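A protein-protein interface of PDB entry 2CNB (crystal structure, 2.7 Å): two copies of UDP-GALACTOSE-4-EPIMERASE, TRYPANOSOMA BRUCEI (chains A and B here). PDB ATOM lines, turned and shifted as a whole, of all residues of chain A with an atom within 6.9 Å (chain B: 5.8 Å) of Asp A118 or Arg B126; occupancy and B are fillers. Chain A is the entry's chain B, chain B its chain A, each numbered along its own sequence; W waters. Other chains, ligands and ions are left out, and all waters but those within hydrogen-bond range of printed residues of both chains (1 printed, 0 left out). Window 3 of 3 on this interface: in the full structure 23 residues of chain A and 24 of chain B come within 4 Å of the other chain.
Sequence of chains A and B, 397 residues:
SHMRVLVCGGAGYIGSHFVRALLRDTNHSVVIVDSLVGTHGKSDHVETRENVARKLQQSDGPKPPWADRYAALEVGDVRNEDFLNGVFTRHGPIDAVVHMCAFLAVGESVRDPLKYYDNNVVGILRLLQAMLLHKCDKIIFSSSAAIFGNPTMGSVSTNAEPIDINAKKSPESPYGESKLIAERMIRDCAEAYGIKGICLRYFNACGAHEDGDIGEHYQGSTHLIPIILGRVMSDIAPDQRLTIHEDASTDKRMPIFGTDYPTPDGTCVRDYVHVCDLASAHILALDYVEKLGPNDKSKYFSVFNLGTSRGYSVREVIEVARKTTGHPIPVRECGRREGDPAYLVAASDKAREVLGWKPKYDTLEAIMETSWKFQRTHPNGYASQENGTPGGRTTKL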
ATOM      1  N   ARG A  79      25.127  -5.062  -6.198  1.00  0.00           N
ATOM      2  CA  ARG A  79      24.664  -4.431  -7.432  1.00  0.00           C
ATOM      3  C   ARG A  79      23.567  -5.231  -8.121  1.00  0.00           C
ATOM      4  O   ARG A  79      22.868  -4.706  -8.991  1.00  0.00           O
ATOM      5  CB  ARG A  79      25.827  -4.182  -8.385  1.00  0.00           C
ATOM      6  CG  ARG A  79      26.693  -3.014  -7.980  1.00  0.00           C
ATOM      7  CD  ARG A  79      27.869  -2.879  -8.892  1.00  0.00           C
ATOM      8  NE  ARG A  79      28.743  -4.051  -8.852  1.00  0.00           N
ATOM      9  CZ  ARG A  79      29.887  -4.145  -9.521  1.00  0.00           C
ATOM     10  NH1 ARG A  79      30.303  -3.139 -10.290  1.00  0.00           N
ATOM     11  NH2 ARG A  79      30.623  -5.240  -9.420  1.00  0.00           N
ATOM     12  N   PHE A 103      36.004  -1.327  -4.401  1.00  0.00           N
ATOM     13  CA  PHE A 103      37.364  -1.614  -4.863  1.00  0.00           C
ATOM     14  C   PHE A 103      38.194  -0.478  -4.313  1.00  0.00           C
ATOM     15  O   PHE A 103      37.670   0.625  -4.121  1.00  0.00           O
ATOM     16  CB  PHE A 103      37.456  -1.689  -6.390  1.00  0.00           C
ATOM     17  CG  PHE A 103      36.730  -2.869  -6.994  1.00  0.00           C
ATOM     18  CD1 PHE A 103      36.757  -4.121  -6.383  1.00  0.00           C
ATOM     19  CD2 PHE A 103      36.036  -2.734  -8.186  1.00  0.00           C
ATOM     20  CE1 PHE A 103      36.077  -5.214  -6.937  1.00  0.00           C
ATOM     21  CE2 PHE A 103      35.361  -3.825  -8.746  1.00  0.00           C
ATOM     22  CZ  PHE A 103      35.384  -5.066  -8.107  1.00  0.00           C
ATOM     23  N   PRO A 113      39.314   3.957 -14.145  1.00  0.00           N
ATOM     24  CA  PRO A 113      38.321   4.583 -13.290  1.00  0.00           C
ATOM     25  C   PRO A 113      36.947   3.935 -13.319  1.00  0.00           C
ATOM     26  O   PRO A 113      36.309   3.823 -12.258  1.00  0.00           O
ATOM     27  CB  PRO A 113      38.235   6.015 -13.832  1.00  0.00           C
ATOM     28  CG  PRO A 113      38.794   5.969 -15.160  1.00  0.00           C
ATOM     29  CD  PRO A 113      39.835   4.911 -15.138  1.00  0.00           C
ATOM     30  N   LEU A 114      36.494   3.508 -14.493  1.00  0.00           N
ATOM     31  CA  LEU A 114      35.127   3.070 -14.641  1.00  0.00           C
ATOM     32  C   LEU A 114      34.886   1.849 -13.790  1.00  0.00           C
ATOM     33  O   LEU A 114      33.777   1.649 -13.296  1.00  0.00           O
ATOM     34  CB  LEU A 114      34.772   2.830 -16.113  1.00  0.00           C
ATOM     35  CG  LEU A 114      34.762   4.058 -17.052  1.00  0.00           C
ATOM     36  CD1 LEU A 114      34.649   3.644 -18.513  1.00  0.00           C
ATOM     37  CD2 LEU A 114      33.659   5.052 -16.690  1.00  0.00           C
ATOM     38  N   LYS A 115      35.928   1.043 -13.587  1.00  0.00           N
ATOM     39  CA  LYS A 115      35.835  -0.130 -12.710  1.00  0.00           C
ATOM     40  C   LYS A 115      35.459   0.295 -11.297  1.00  0.00           C
ATOM     41  O   LYS A 115      34.675  -0.380 -10.632  1.00  0.00           O
ATOM     42  CB  LYS A 115      37.163  -0.902 -12.694  1.00  0.00           C
ATOM     43  CG  LYS A 115      37.189  -2.122 -11.758  1.00  0.00           C
ATOM     44  CD  LYS A 115      38.585  -2.743 -11.622  1.00  0.00           C
ATOM     45  CE  LYS A 115      38.558  -3.907 -10.626  1.00  0.00           C
ATOM     46  NZ  LYS A 115      39.829  -4.706 -10.634  1.00  0.00           N
ATOM     47  N   TYR A 116      36.033   1.420 -10.866  1.00  0.00           N
ATOM     48  CA  TYR A 116      35.814   1.993  -9.537  1.00  0.00           C
ATOM     49  C   TYR A 116      34.503   2.754  -9.461  1.00  0.00           C
ATOM     50  O   TYR A 116      33.780   2.663  -8.463  1.00  0.00           O
ATOM     51  CB  TYR A 116      37.000   2.870  -9.114  1.00  0.00           C
ATOM     52  CG  TYR A 116      38.158   2.025  -8.618  1.00  0.00           C
ATOM     53  CD1 TYR A 116      38.911   1.241  -9.508  1.00  0.00           C
ATOM     54  CD2 TYR A 116      38.474   1.959  -7.261  1.00  0.00           C
ATOM     55  CE1 TYR A 116      39.957   0.442  -9.072  1.00  0.00           C
ATOM     56  CE2 TYR A 116      39.521   1.161  -6.818  1.00  0.00           C
ATOM     57  CZ  TYR A 116      40.254   0.400  -7.737  1.00  0.00           C
ATOM     58  OH  TYR A 116      41.280  -0.396  -7.312  1.00  0.00           O
ATOM     59  N   TYR A 117      34.192   3.488 -10.525  1.00  0.00           N
ATOM     60  CA  TYR A 117      32.962   4.241 -10.584  1.00  0.00           C
ATOM     61  C   TYR A 117      31.776   3.295 -10.606  1.00  0.00           C
ATOM     62  O   TYR A 117      30.748   3.548  -9.986  1.00  0.00           O
ATOM     63  CB  TYR A 117      32.955   5.094 -11.827  1.00  0.00           C
ATOM     64  CG  TYR A 117      33.731   6.371 -11.665  1.00  0.00           C
ATOM     65  CD1 TYR A 117      33.339   7.323 -10.724  1.00  0.00           C
ATOM     66  CD2 TYR A 117      34.850   6.651 -12.470  1.00  0.00           C
ATOM     67  CE1 TYR A 117      34.026   8.512 -10.578  1.00  0.00           C
ATOM     68  CE2 TYR A 117      35.544   7.848 -12.324  1.00  0.00           C
ATOM     69  CZ  TYR A 117      35.123   8.773 -11.368  1.00  0.00           C
ATOM     70  OH  TYR A 117      35.794   9.969 -11.194  1.00  0.00           O
ATOM     71  N   ASP A 118      31.920   2.199 -11.326  1.00  0.00           N
ATOM     72  CA  ASP A 118      30.850   1.240 -11.406  1.00  0.00           C
ATOM     73  C   ASP A 118      30.627   0.696  -9.994  1.00  0.00           C
ATOM     74  O   ASP A 118      29.613   1.014  -9.362  1.00  0.00           O
ATOM     75  CB  ASP A 118      31.190   0.138 -12.422  1.00  0.00           C
ATOM     76  CG  ASP A 118      30.004  -0.748 -12.742  1.00  0.00           C
ATOM     77  OD1 ASP A 118      29.208  -1.021 -11.812  1.00  0.00           O
ATOM     78  OD2 ASP A 118      29.871  -1.186 -13.916  1.00  0.00           O
ATOM     79  N   ASN A 119      31.602  -0.065  -9.483  1.00  0.00           N
ATOM     80  CA  ASN A 119      31.502  -0.679  -8.156  1.00  0.00           C
ATOM     81  C   ASN A 119      31.251   0.280  -6.995  1.00  0.00           C
ATOM     82  O   ASN A 119      30.245   0.166  -6.326  1.00  0.00           O
ATOM     83  CB  ASN A 119      32.716  -1.547  -7.865  1.00  0.00           C
ATOM     84  CG  ASN A 119      32.456  -2.552  -6.745  1.00  0.00           C
ATOM     85  OD1 ASN A 119      31.327  -2.968  -6.539  1.00  0.00           O
ATOM     86  ND2 ASN A 119      33.513  -2.956  -6.033  1.00  0.00           N
ATOM     87  N   ASN A 120      32.150   1.225  -6.752  1.00  0.00           N
ATOM     88  CA  ASN A 120      31.978   2.122  -5.590  1.00  0.00           C
ATOM     89  C   ASN A 120      30.656   2.898  -5.627  1.00  0.00           C
ATOM     90  O   ASN A 120      29.912   2.885  -4.637  1.00  0.00           O
ATOM     91  CB  ASN A 120      33.164   3.080  -5.374  1.00  0.00           C
ATOM     92  CG  ASN A 120      34.490   2.353  -5.151  1.00  0.00           C
ATOM     93  OD1 ASN A 120      34.548   1.116  -5.159  1.00  0.00           O
ATOM     94  ND2 ASN A 120      35.568   3.124  -4.965  1.00  0.00           N
ATOM     95  N   VAL A 121      30.356   3.528  -6.767  1.00  0.00           N
ATOM     96  CA  VAL A 121      29.187   4.409  -6.885  1.00  0.00           C
ATOM     97  C   VAL A 121      27.874   3.653  -7.124  1.00  0.00           C
ATOM     98  O   VAL A 121      26.882   3.902  -6.425  1.00  0.00           O
ATOM     99  CB  VAL A 121      29.383   5.514  -7.942  1.00  0.00           C
ATOM    100  CG1 VAL A 121      28.145   6.402  -8.033  1.00  0.00           C
ATOM    101  CG2 VAL A 121      30.585   6.347  -7.595  1.00  0.00           C
ATOM    102  N   VAL A 122      27.856   2.728  -8.082  1.00  0.00           N
ATOM    103  CA  VAL A 122      26.630   1.984  -8.337  1.00  0.00           C
ATOM    104  C   VAL A 122      26.264   1.179  -7.093  1.00  0.00           C
ATOM    105  O   VAL A 122      25.074   1.048  -6.749  1.00  0.00           O
ATOM    106  CB  VAL A 122      26.705   1.126  -9.625  1.00  0.00           C
ATOM    107  CG1 VAL A 122      25.542   0.137  -9.733  1.00  0.00           C
ATOM    108  CG2 VAL A 122      26.681   2.031 -10.804  1.00  0.00           C
ATOM    109  N   GLY A 123      27.293   0.682  -6.411  1.00  0.00           N
ATOM    110  CA  GLY A 123      27.128  -0.035  -5.147  1.00  0.00           C
ATOM    111  C   GLY A 123      26.336   0.745  -4.114  1.00  0.00           C
ATOM    112  O   GLY A 123      25.313   0.269  -3.656  1.00  0.00           O
ATOM    113  N   ILE A 124      26.787   1.946  -3.757  1.00  0.00           N
ATOM    114  CA  ILE A 124      26.097   2.734  -2.746  1.00  0.00           C
ATOM    115  C   ILE A 124      24.696   3.147  -3.168  1.00  0.00           C
ATOM    116  O   ILE A 124      23.823   3.305  -2.310  1.00  0.00           O
ATOM    117  CB  ILE A 124      26.884   3.982  -2.314  1.00  0.00           C
ATOM    118  CG1 ILE A 124      26.224   4.636  -1.095  1.00  0.00           C
ATOM    119  CG2 ILE A 124      27.006   4.995  -3.445  1.00  0.00           C
ATOM    120  CD1 ILE A 124      26.139   3.736   0.118  1.00  0.00           C
ATOM    121  N   ARG A 126      22.592   1.349  -5.049  1.00  0.00           N
ATOM    122  CA  ARG A 126      21.699   0.226  -4.951  1.00  0.00           C
ATOM    123  C   ARG A 126      21.257   0.113  -3.515  1.00  0.00           C
ATOM    124  O   ARG A 126      20.057   0.070  -3.239  1.00  0.00           O
ATOM    125  CB  ARG A 126      22.365  -1.045  -5.464  1.00  0.00           C
ATOM    126  CG  ARG A 126      22.651  -0.999  -6.967  1.00  0.00           C
ATOM    127  CD  ARG A 126      21.487  -0.337  -7.664  1.00  0.00           C
ATOM    128  NE  ARG A 126      21.548  -0.357  -9.121  1.00  0.00           N
ATOM    129  CZ  ARG A 126      20.865   0.491  -9.883  1.00  0.00           C
ATOM    130  NH1 ARG A 126      20.107   1.414  -9.296  1.00  0.00           N
ATOM    131  NH2 ARG A 126      20.950   0.437 -11.214  1.00  0.00           N
ATOM    132  N   VAL B  78      19.484   3.896 -22.200  1.00  0.00           N
ATOM    133  CA  VAL B  78      20.947   3.700 -22.256  1.00  0.00           C
ATOM    134  C   VAL B  78      21.470   2.929 -21.059  1.00  0.00           C
ATOM    135  O   VAL B  78      22.508   2.292 -21.140  1.00  0.00           O
ATOM    136  CB  VAL B  78      21.761   5.032 -22.402  1.00  0.00           C
ATOM    137  CG1 VAL B  78      21.642   5.591 -23.813  1.00  0.00           C
ATOM    138  CG2 VAL B  78      21.365   6.069 -21.340  1.00  0.00           C
ATOM    139  N   ARG B  79      20.765   3.017 -19.938  1.00  0.00           N
ATOM    140  CA  ARG B  79      21.044   2.144 -18.792  1.00  0.00           C
ATOM    141  C   ARG B  79      20.929   0.647 -19.108  1.00  0.00           C
ATOM    142  O   ARG B  79      21.558  -0.155 -18.438  1.00  0.00           O
ATOM    143  CB  ARG B  79      20.176   2.518 -17.599  1.00  0.00           C
ATOM    144  CG  ARG B  79      20.665   3.751 -16.888  1.00  0.00           C
ATOM    145  CD  ARG B  79      19.720   4.150 -15.790  1.00  0.00           C
ATOM    146  NE  ARG B  79      18.367   4.286 -16.311  1.00  0.00           N
ATOM    147  CZ  ARG B  79      17.341   4.828 -15.664  1.00  0.00           C
ATOM    148  NH1 ARG B  79      17.460   5.304 -14.419  1.00  0.00           N
ATOM    149  NH2 ARG B  79      16.178   4.887 -16.286  1.00  0.00           N
ATOM    150  N   ASN B  80      20.138   0.285 -20.119  1.00  0.00           N
ATOM    151  CA  ASN B  80      20.113  -1.075 -20.647  1.00  0.00           C
ATOM    152  C   ASN B  80      21.321  -1.392 -21.543  1.00  0.00           C
ATOM    153  O   ASN B  80      21.348  -1.085 -22.749  1.00  0.00           O
ATOM    154  CB  ASN B  80      18.828  -1.310 -21.421  1.00  0.00           C
ATOM    155  CG  ASN B  80      18.596  -2.773 -21.764  1.00  0.00           C
ATOM    156  OD1 ASN B  80      17.457  -3.197 -21.863  1.00  0.00           O
ATOM    157  ND2 ASN B  80      19.655  -3.542 -21.943  1.00  0.00           N
ATOM    158  N   GLU B  81      22.293  -2.051 -20.920  1.00  0.00           N
ATOM    159  CA  GLU B  81      23.596  -2.410 -21.503  1.00  0.00           C
ATOM    160  C   GLU B  81      23.472  -3.350 -22.702  1.00  0.00           C
ATOM    161  O   GLU B  81      24.297  -3.364 -23.626  1.00  0.00           O
ATOM    162  CB  GLU B  81      24.466  -3.056 -20.405  1.00  0.00           C
ATOM    163  CG  GLU B  81      24.726  -2.129 -19.184  1.00  0.00           C
ATOM    164  CD  GLU B  81      25.022  -2.896 -17.900  1.00  0.00           C
ATOM    165  OE1 GLU B  81      26.158  -2.769 -17.380  1.00  0.00           O
ATOM    166  OE2 GLU B  81      24.118  -3.632 -17.421  1.00  0.00           O
ATOM    167  N   LEU B  84      21.924  -1.213 -25.528  1.00  0.00           N
ATOM    168  CA  LEU B  84      22.841  -0.168 -25.935  1.00  0.00           C
ATOM    169  C   LEU B  84      23.975  -0.774 -26.748  1.00  0.00           C
ATOM    170  O   LEU B  84      24.400  -0.232 -27.773  1.00  0.00           O
ATOM    171  CB  LEU B  84      23.367   0.598 -24.710  1.00  0.00           C
ATOM    172  CG  LEU B  84      24.324   1.768 -24.975  1.00  0.00           C
ATOM    173  CD1 LEU B  84      23.613   2.922 -25.638  1.00  0.00           C
ATOM    174  CD2 LEU B  84      24.952   2.209 -23.703  1.00  0.00           C
ATOM    175  N   VAL B 121      23.759   9.682 -13.427  1.00  0.00           N
ATOM    176  CA  VAL B 121      25.085   9.107 -13.252  1.00  0.00           C
ATOM    177  C   VAL B 121      25.214   7.725 -13.907  1.00  0.00           C
ATOM    178  O   VAL B 121      26.154   7.490 -14.673  1.00  0.00           O
ATOM    179  CB  VAL B 121      25.512   9.043 -11.789  1.00  0.00           C
ATOM    180  CG1 VAL B 121      26.948   8.531 -11.703  1.00  0.00           C
ATOM    181  CG2 VAL B 121      25.367  10.411 -11.128  1.00  0.00           C
ATOM    182  N   VAL B 122      24.285   6.815 -13.611  1.00  0.00           N
ATOM    183  CA  VAL B 122      24.366   5.466 -14.180  1.00  0.00           C
ATOM    184  C   VAL B 122      24.296   5.499 -15.711  1.00  0.00           C
ATOM    185  O   VAL B 122      24.987   4.738 -16.383  1.00  0.00           O
ATOM    186  CB  VAL B 122      23.317   4.486 -13.585  1.00  0.00           C
ATOM    187  CG1 VAL B 122      23.367   3.123 -14.307  1.00  0.00           C
ATOM    188  CG2 VAL B 122      23.583   4.282 -12.108  1.00  0.00           C
ATOM    189  N   GLY B 123      23.480   6.398 -16.251  1.00  0.00           N
ATOM    190  CA  GLY B 123      23.399   6.578 -17.696  1.00  0.00           C
ATOM    191  C   GLY B 123      24.773   6.843 -18.294  1.00  0.00           C
ATOM    192  O   GLY B 123      25.235   6.084 -19.141  1.00  0.00           O
ATOM    193  N   ILE B 124      25.437   7.900 -17.832  1.00  0.00           N
ATOM    194  CA  ILE B 124      26.745   8.263 -18.347  1.00  0.00           C
ATOM    195  C   ILE B 124      27.754   7.106 -18.205  1.00  0.00           C
ATOM    196  O   ILE B 124      28.525   6.814 -19.150  1.00  0.00           O
ATOM    197  CB  ILE B 124      27.270   9.572 -17.712  1.00  0.00           C
ATOM    198  CG1 ILE B 124      28.602  10.001 -18.331  1.00  0.00           C
ATOM    199  CG2 ILE B 124      27.451   9.412 -16.236  1.00  0.00           C
ATOM    200  CD1 ILE B 124      28.592  10.134 -19.827  1.00  0.00           C
ATOM    201  N   LEU B 125      27.722   6.438 -17.048  1.00  0.00           N
ATOM    202  CA  LEU B 125      28.651   5.354 -16.756  1.00  0.00           C
ATOM    203  C   LEU B 125      28.546   4.230 -17.795  1.00  0.00           C
ATOM    204  O   LEU B 125      29.549   3.594 -18.152  1.00  0.00           O
ATOM    205  CB  LEU B 125      28.403   4.822 -15.351  1.00  0.00           C
ATOM    206  CG  LEU B 125      29.091   3.497 -15.016  1.00  0.00           C
ATOM    207  CD1 LEU B 125      30.562   3.726 -14.748  1.00  0.00           C
ATOM    208  CD2 LEU B 125      28.400   2.777 -13.839  1.00  0.00           C
ATOM    209  N   ARG B 126      27.327   4.019 -18.289  1.00  0.00           N
ATOM    210  CA  ARG B 126      27.047   2.973 -19.263  1.00  0.00           C
ATOM    211  C   ARG B 126      27.538   3.380 -20.639  1.00  0.00           C
ATOM    212  O   ARG B 126      28.069   2.550 -21.385  1.00  0.00           O
ATOM    213  CB  ARG B 126      25.552   2.640 -19.303  1.00  0.00           C
ATOM    214  CG  ARG B 126      24.994   2.039 -18.024  1.00  0.00           C
ATOM    215  CD  ARG B 126      25.986   1.071 -17.402  1.00  0.00           C
ATOM    216  NE  ARG B 126      25.480   0.441 -16.185  1.00  0.00           N
ATOM    217  CZ  ARG B 126      26.251  -0.152 -15.273  1.00  0.00           C
ATOM    218  NH1 ARG B 126      27.565  -0.195 -15.418  1.00  0.00           N
ATOM    219  NH2 ARG B 126      25.714  -0.704 -14.211  1.00  0.00           N
ATOM    220  N   LEU B 127      27.366   4.660 -20.964  1.00  0.00           N
ATOM    221  CA  LEU B 127      27.896   5.197 -22.201  1.00  0.00           C
ATOM    222  C   LEU B 127      29.384   5.019 -22.257  1.00  0.00           C
ATOM    223  O   LEU B 127      29.915   4.538 -23.250  1.00  0.00           O
ATOM    224  CB  LEU B 127      27.574   6.686 -22.380  1.00  0.00           C
ATOM    225  CG  LEU B 127      26.724   6.897 -23.634  1.00  0.00           C
ATOM    226  CD1 LEU B 127      27.357   6.232 -24.841  1.00  0.00           C
ATOM    227  CD2 LEU B 127      25.327   6.330 -23.423  1.00  0.00           C
ATOM    228  N   LEU B 128      30.068   5.414 -21.195  1.00  0.00           N
ATOM    229  CA  LEU B 128      31.504   5.402 -21.249  1.00  0.00           C
ATOM    230  C   LEU B 128      31.961   3.964 -21.384  1.00  0.00           C
ATOM    231  O   LEU B 128      32.922   3.678 -22.090  1.00  0.00           O
ATOM    232  CB  LEU B 128      32.094   6.095 -20.033  1.00  0.00           C
ATOM    233  CG  LEU B 128      31.771   7.593 -20.004  1.00  0.00           C
ATOM    234  CD1 LEU B 128      31.869   8.201 -18.591  1.00  0.00           C
ATOM    235  CD2 LEU B 128      32.657   8.319 -20.986  1.00  0.00           C
ATOM    236  N   GLN B 129      31.235   3.053 -20.748  1.00  0.00           N
ATOM    237  CA  GLN B 129      31.593   1.638 -20.802  1.00  0.00           C
ATOM    238  C   GLN B 129      31.400   1.062 -22.194  1.00  0.00           C
ATOM    239  O   GLN B 129      32.272   0.361 -22.700  1.00  0.00           O
ATOM    240  CB  GLN B 129      30.835   0.851 -19.753  1.00  0.00           C
ATOM    241  CG  GLN B 129      31.446   1.081 -18.403  1.00  0.00           C
ATOM    242  CD  GLN B 129      30.692   0.426 -17.295  1.00  0.00           C
ATOM    243  OE1 GLN B 129      29.478   0.248 -17.362  1.00  0.00           O
ATOM    244  NE2 GLN B 129      31.416   0.048 -16.253  1.00  0.00           N
ATOM    245  N   ALA B 130      30.275   1.408 -22.812  1.00  0.00           N
ATOM    246  CA  ALA B 130      29.984   1.036 -24.186  1.00  0.00           C
ATOM    247  C   ALA B 130      31.016   1.601 -25.155  1.00  0.00           C
ATOM    248  O   ALA B 130      31.528   0.880 -26.020  1.00  0.00           O
ATOM    249  CB  ALA B 130      28.598   1.489 -24.561  1.00  0.00           C
ATOM    250  N   MET B 131      31.323   2.885 -25.016  1.00  0.00           N
ATOM    251  CA  MET B 131      32.362   3.487 -25.837  1.00  0.00           C
ATOM    252  C   MET B 131      33.639   2.654 -25.747  1.00  0.00           C
ATOM    253  O   MET B 131      34.228   2.291 -26.763  1.00  0.00           O
ATOM    254  CB  MET B 131      32.629   4.910 -25.414  1.00  0.00           C
ATOM    255  CG  MET B 131      31.497   5.829 -25.710  1.00  0.00           C
ATOM    256  SD  MET B 131      31.803   7.446 -24.992  1.00  0.00           S
ATOM    257  CE  MET B 131      33.391   7.879 -25.687  1.00  0.00           C
HETATM  258  O   HOH W   1      27.044  -2.153 -12.039  1.00  0.00           O
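The guanidinium group (NH1) of Arg B126 lies within salt-bridge range of the side-chain carboxylate (OD2) of Asp A118 (2.9 Å). The side-chain carboxylate (OD2) of Asp A118 is in hydrogen-bond range of the side-chain amide nitrogen (NE2) of Gln B129 (3.1 Å).
Of the 15 printed residues of chain A, 3 touch a printed residue of chain B. Hydrophobic or aromatic side chains of chain A that line the printed part of chain B: Leu A114 and Val A122. Among the printed residues, 6 pairs touch across the chains. Among the printed residues, Asp or Glu carboxylates within 4 Å of a Lys or Arg side-chain nitrogen of the other chain: Asp A118 with Arg B126 (2.9 Å).
OE1 of Glu B81 is in salt-bridge range of NE of Arg B126 (3.5 Å). The backbone carbonyl oxygen (O) of Leu B125 lies close to the side-chain amide oxygen (OE1) of Gln B129, 3.4 Å away. The side-chain amide oxygen of Gln B129 sits at hydrogen-bond distance from the guanidinium group of Arg B126. NH1 of Arg A79 lies within salt-bridge range of OD1 of Asp A118 (2.8 Å).
Leu B125 touches Leu A114. Leu A114 touches Leu B128 (CD2 to CB, 3.8 Å). Leu B125 touches Asp A118 (CD2 to CA, 3.8 Å). Leu B125 touches Val A122.
6 positions are printed for both chains. Of the 6 pairs that touch across the chains among the printed residues, none has its exchanged pair printed and touching as well.
Of the printed residues of chain B, Leu A114 touches Leu B125 and Leu B128. Asp A118 touches three residues of chain B. Of the printed residues of chain B, Val A122 touches Leu B125. Of the printed residues of chain A, Leu B125 touches Leu A114 (3.9 Å), Asp A118 (3.8 Å) and Val A122 (3.6 Å). Of the printed residues of chain A, Leu B128 touches Leu A114. Of the printed residues of chain A, Gln B129 touches Asp A118. The nearest residue of chain A that does not touch Arg B126 is Val A122 (4.5 Å).
Water W1 lies within hydrogen-bond range of the side-chain carboxylate of Asp A118 (2.5 Å) and the guanidinium group of Arg B126 (2.9 Å).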
